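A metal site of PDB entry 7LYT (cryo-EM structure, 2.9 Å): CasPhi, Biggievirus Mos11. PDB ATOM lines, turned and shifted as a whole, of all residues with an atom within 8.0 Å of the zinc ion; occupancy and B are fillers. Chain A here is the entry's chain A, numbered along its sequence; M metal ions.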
ATOM      1  N   ILE A 665      14.196 -12.473 -11.315  1.00  0.00           N
ATOM      2  CA  ILE A 665      14.218 -11.298 -12.169  1.00  0.00           C
ATOM      3  C   ILE A 665      14.614 -10.045 -11.396  1.00  0.00           C
ATOM      4  O   ILE A 665      15.527  -9.312 -11.793  1.00  0.00           O
ATOM      5  CB  ILE A 665      12.852 -11.084 -12.873  1.00  0.00           C
ATOM      6  CG1 ILE A 665      12.633 -12.178 -13.916  1.00  0.00           C
ATOM      7  CG2 ILE A 665      12.796  -9.695 -13.497  1.00  0.00           C
ATOM      8  CD1 ILE A 665      11.244 -12.173 -14.519  1.00  0.00           C
ATOM      9  N   THR A 666      13.936  -9.770 -10.279  1.00  0.00           N
ATOM     10  CA  THR A 666      14.080  -8.478  -9.617  1.00  0.00           C
ATOM     11  C   THR A 666      15.529  -8.246  -9.219  1.00  0.00           C
ATOM     12  O   THR A 666      16.107  -9.018  -8.450  1.00  0.00           O
ATOM     13  CB  THR A 666      13.181  -8.423  -8.387  1.00  0.00           C
ATOM     14  OG1 THR A 666      11.807  -8.440  -8.790  1.00  0.00           O
ATOM     15  CG2 THR A 666      13.447  -7.149  -7.582  1.00  0.00           C
ATOM     16  N   CYS A 667      16.118  -7.190  -9.770  1.00  0.00           N
ATOM     17  CA  CYS A 667      17.474  -6.804  -9.398  1.00  0.00           C
ATOM     18  C   CYS A 667      17.604  -6.746  -7.878  1.00  0.00           C
ATOM     19  O   CYS A 667      16.718  -6.211  -7.204  1.00  0.00           O
ATOM     20  CB  CYS A 667      17.820  -5.447 -10.005  1.00  0.00           C
ATOM     21  SG  CYS A 667      19.532  -4.950  -9.687  1.00  0.00           S
ATOM     22  N   PRO A 668      18.684  -7.290  -7.311  1.00  0.00           N
ATOM     23  CA  PRO A 668      18.869  -7.158  -5.855  1.00  0.00           C
ATOM     24  C   PRO A 668      18.922  -5.711  -5.392  1.00  0.00           C
ATOM     25  O   PRO A 668      18.274  -5.363  -4.390  1.00  0.00           O
ATOM     26  CB  PRO A 668      20.198  -7.887  -5.606  1.00  0.00           C
ATOM     27  CG  PRO A 668      20.362  -8.797  -6.773  1.00  0.00           C
ATOM     28  CD  PRO A 668      19.761  -8.091  -7.931  1.00  0.00           C
ATOM     29  N   LYS A 669      19.692  -4.863  -6.079  1.00  0.00           N
ATOM     30  CA  LYS A 669      19.922  -3.511  -5.586  1.00  0.00           C
ATOM     31  C   LYS A 669      18.670  -2.638  -5.705  1.00  0.00           C
ATOM     32  O   LYS A 669      18.358  -1.885  -4.771  1.00  0.00           O
ATOM     33  CB  LYS A 669      21.066  -2.865  -6.368  1.00  0.00           C
ATOM     34  CG  LYS A 669      22.365  -3.641  -6.314  1.00  0.00           C
ATOM     35  CD  LYS A 669      23.480  -2.914  -7.044  1.00  0.00           C
ATOM     36  CE  LYS A 669      23.965  -1.696  -6.273  1.00  0.00           C
ATOM     37  NZ  LYS A 669      24.825  -0.837  -7.109  1.00  0.00           N
ATOM     38  N   CYS A 670      17.952  -2.729  -6.817  1.00  0.00           N
ATOM     39  CA  CYS A 670      16.861  -1.814  -7.111  1.00  0.00           C
ATOM     40  C   CYS A 670      15.572  -2.576  -7.375  1.00  0.00           C
ATOM     41  O   CYS A 670      15.585  -3.716  -7.852  1.00  0.00           O
ATOM     42  CB  CYS A 670      17.179  -0.932  -8.323  1.00  0.00           C
ATOM     43  SG  CYS A 670      17.325  -1.837  -9.873  1.00  0.00           S
ATOM     44  N   GLY A 671      14.450  -1.924  -7.067  1.00  0.00           N
ATOM     45  CA  GLY A 671      13.128  -2.522  -7.131  1.00  0.00           C
ATOM     46  C   GLY A 671      12.544  -2.659  -8.519  1.00  0.00           C
ATOM     47  O   GLY A 671      11.321  -2.768  -8.676  1.00  0.00           O
ATOM     48  N   HIS A 672      13.390  -2.660  -9.545  1.00  0.00           N
ATOM     49  CA  HIS A 672      12.947  -2.663 -10.935  1.00  0.00           C
ATOM     50  C   HIS A 672      13.022  -4.093 -11.456  1.00  0.00           C
ATOM     51  O   HIS A 672      14.082  -4.726 -11.418  1.00  0.00           O
ATOM     52  CB  HIS A 672      13.813  -1.728 -11.775  1.00  0.00           C
ATOM     53  CG  HIS A 672      13.488  -1.740 -13.240  1.00  0.00           C
ATOM     54  ND1 HIS A 672      14.273  -2.381 -14.167  1.00  0.00           N
ATOM     55  CD2 HIS A 672      12.460  -1.179 -13.915  1.00  0.00           C
ATOM     56  CE1 HIS A 672      13.739  -2.209 -15.363  1.00  0.00           C
ATOM     57  NE2 HIS A 672      12.643  -1.487 -15.243  1.00  0.00           N
ATOM     58  N   CYS A 673      11.883  -4.597 -11.941  1.00  0.00           N
ATOM     59  CA  CYS A 673      11.660  -6.028 -12.127  1.00  0.00           C
ATOM     60  C   CYS A 673      11.453  -6.422 -13.582  1.00  0.00           C
ATOM     61  O   CYS A 673      10.929  -7.504 -13.857  1.00  0.00           O
ATOM     62  CB  CYS A 673      10.470  -6.486 -11.287  1.00  0.00           C
ATOM     63  SG  CYS A 673       8.944  -5.576 -11.613  1.00  0.00           S
ATOM     64  N   ASN A 677      15.855  -8.443 -17.768  1.00  0.00           N
ATOM     65  CA  ASN A 677      17.140  -8.490 -17.082  1.00  0.00           C
ATOM     66  C   ASN A 677      17.730  -9.894 -17.113  1.00  0.00           C
ATOM     67  O   ASN A 677      18.920 -10.074 -17.366  1.00  0.00           O
ATOM     68  CB  ASN A 677      16.979  -8.023 -15.638  1.00  0.00           C
ATOM     69  CG  ASN A 677      16.300  -6.673 -15.527  1.00  0.00           C
ATOM     70  OD1 ASN A 677      16.949  -5.628 -15.654  1.00  0.00           O
ATOM     71  ND2 ASN A 677      15.002  -6.681 -15.283  1.00  0.00           N
ATOM     72  N   PHE A 683      22.587 -12.854 -15.483  1.00  0.00           N
ATOM     73  CA  PHE A 683      21.680 -11.763 -15.156  1.00  0.00           C
ATOM     74  C   PHE A 683      22.374 -10.430 -15.392  1.00  0.00           C
ATOM     75  O   PHE A 683      23.587 -10.293 -15.199  1.00  0.00           O
ATOM     76  CB  PHE A 683      21.214 -11.860 -13.702  1.00  0.00           C
ATOM     77  CG  PHE A 683      20.586 -10.599 -13.178  1.00  0.00           C
ATOM     78  CD1 PHE A 683      21.365  -9.607 -12.600  1.00  0.00           C
ATOM     79  CD2 PHE A 683      19.221 -10.401 -13.251  1.00  0.00           C
ATOM     80  CE1 PHE A 683      20.799  -8.455 -12.112  1.00  0.00           C
ATOM     81  CE2 PHE A 683      18.646  -9.243 -12.762  1.00  0.00           C
ATOM     82  CZ  PHE A 683      19.435  -8.270 -12.192  1.00  0.00           C
ATOM     83  N   GLN A 684      21.597  -9.436 -15.812  1.00  0.00           N
ATOM     84  CA  GLN A 684      22.124  -8.079 -15.953  1.00  0.00           C
ATOM     85  C   GLN A 684      20.969  -7.101 -15.831  1.00  0.00           C
ATOM     86  O   GLN A 684      20.144  -7.006 -16.745  1.00  0.00           O
ATOM     87  CB  GLN A 684      22.850  -7.915 -17.282  1.00  0.00           C
ATOM     88  CG  GLN A 684      23.719  -6.670 -17.347  1.00  0.00           C
ATOM     89  CD  GLN A 684      24.053  -6.273 -18.766  1.00  0.00           C
ATOM     90  OE1 GLN A 684      23.709  -6.972 -19.721  1.00  0.00           O
ATOM     91  NE2 GLN A 684      24.717  -5.137 -18.909  1.00  0.00           N
ATOM     92  N   CYS A 685      20.924  -6.367 -14.726  1.00  0.00           N
ATOM     93  CA  CYS A 685      19.944  -5.300 -14.589  1.00  0.00           C
ATOM     94  C   CYS A 685      20.142  -4.272 -15.698  1.00  0.00           C
ATOM     95  O   CYS A 685      21.256  -4.023 -16.160  1.00  0.00           O
ATOM     96  CB  CYS A 685      20.049  -4.610 -13.235  1.00  0.00           C
ATOM     97  SG  CYS A 685      18.818  -3.311 -13.009  1.00  0.00           S
ATOM     98  N   LEU A 686      19.028  -3.672 -16.149  1.00  0.00           N
ATOM     99  CA  LEU A 686      19.063  -2.711 -17.235  1.00  0.00           C
ATOM    100  C   LEU A 686      18.908  -1.266 -16.780  1.00  0.00           C
ATOM    101  O   LEU A 686      18.714  -0.388 -17.633  1.00  0.00           O
ATOM    102  CB  LEU A 686      17.978  -3.054 -18.259  1.00  0.00           C
ATOM    103  CG  LEU A 686      17.910  -4.506 -18.716  1.00  0.00           C
ATOM    104  CD1 LEU A 686      16.748  -4.702 -19.673  1.00  0.00           C
ATOM    105  CD2 LEU A 686      19.208  -4.944 -19.368  1.00  0.00           C
ATOM    106  N   SER A 687      18.964  -0.990 -15.479  1.00  0.00           N
ATOM    107  CA  SER A 687      19.082   0.389 -15.006  1.00  0.00           C
ATOM    108  C   SER A 687      20.399   0.680 -14.312  1.00  0.00           C
ATOM    109  O   SER A 687      21.098   1.630 -14.690  1.00  0.00           O
ATOM    110  CB  SER A 687      17.915   0.690 -14.043  1.00  0.00           C
ATOM    111  OG  SER A 687      16.677   0.487 -14.683  1.00  0.00           O
ATOM    112  N   CYS A 688      20.754  -0.116 -13.311  1.00  0.00           N
ATOM    113  CA  CYS A 688      22.055  -0.037 -12.646  1.00  0.00           C
ATOM    114  C   CYS A 688      22.895  -1.209 -13.159  1.00  0.00           C
ATOM    115  O   CYS A 688      22.898  -2.294 -12.563  1.00  0.00           O
ATOM    116  CB  CYS A 688      21.899  -0.067 -11.127  1.00  0.00           C
ATOM    117  SG  CYS A 688      20.990  -1.480 -10.491  1.00  0.00           S
ATOM    118  N   GLY A 689      23.593  -0.999 -14.260  1.00  0.00           N
ATOM    119  CA  GLY A 689      24.243  -2.105 -14.937  1.00  0.00           C
ATOM    120  C   GLY A 689      25.101  -2.917 -13.983  1.00  0.00           C
ATOM    121  O   GLY A 689      25.982  -2.385 -13.313  1.00  0.00           O
ATOM    122  N   LYS A 690      24.824  -4.220 -13.935  1.00  0.00           N
ATOM    123  CA  LYS A 690      25.377  -5.108 -12.934  1.00  0.00           C
ATOM    124  C   LYS A 690      25.316  -6.521 -13.495  1.00  0.00           C
ATOM    125  O   LYS A 690      24.412  -6.855 -14.257  1.00  0.00           O
ATOM    126  CB  LYS A 690      24.582  -5.008 -11.623  1.00  0.00           C
ATOM    127  CG  LYS A 690      25.002  -5.978 -10.532  1.00  0.00           C
ATOM    128  CD  LYS A 690      24.257  -5.637  -9.252  1.00  0.00           C
ATOM    129  CE  LYS A 690      24.669  -6.536  -8.099  1.00  0.00           C
ATOM    130  NZ  LYS A 690      26.137  -6.498  -7.863  1.00  0.00           N
HETATM  131 ZN    ZN M   1      19.184  -2.912 -10.754  1.00  0.00          ZN
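Four residues have an atom within 4 Å of the zinc ion: Cys 667, Cys 670, Cys 685 and Cys 688. The nearest printed residue that does not touch the zinc ion is Lys 669 (4.8 Å).
The zinc ion is bound by the side-chain sulfur (SG) of Cys 688 (2.3 Å), the side-chain sulfur (SG) of Cys 685 (2.3 Å), the side-chain sulfur (SG) of Cys 670 (2.3 Å) and the side-chain sulfur (SG) of Cys 667 (2.3 Å). The zinc ion has four donor atoms within binding distance.
The backbone NH of Ser 687 sits close to the side-chain sulfur of Cys 685, 3.4 Å away. N of Lys 669 sits close to SG of Cys 667, 3.6 Å away.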
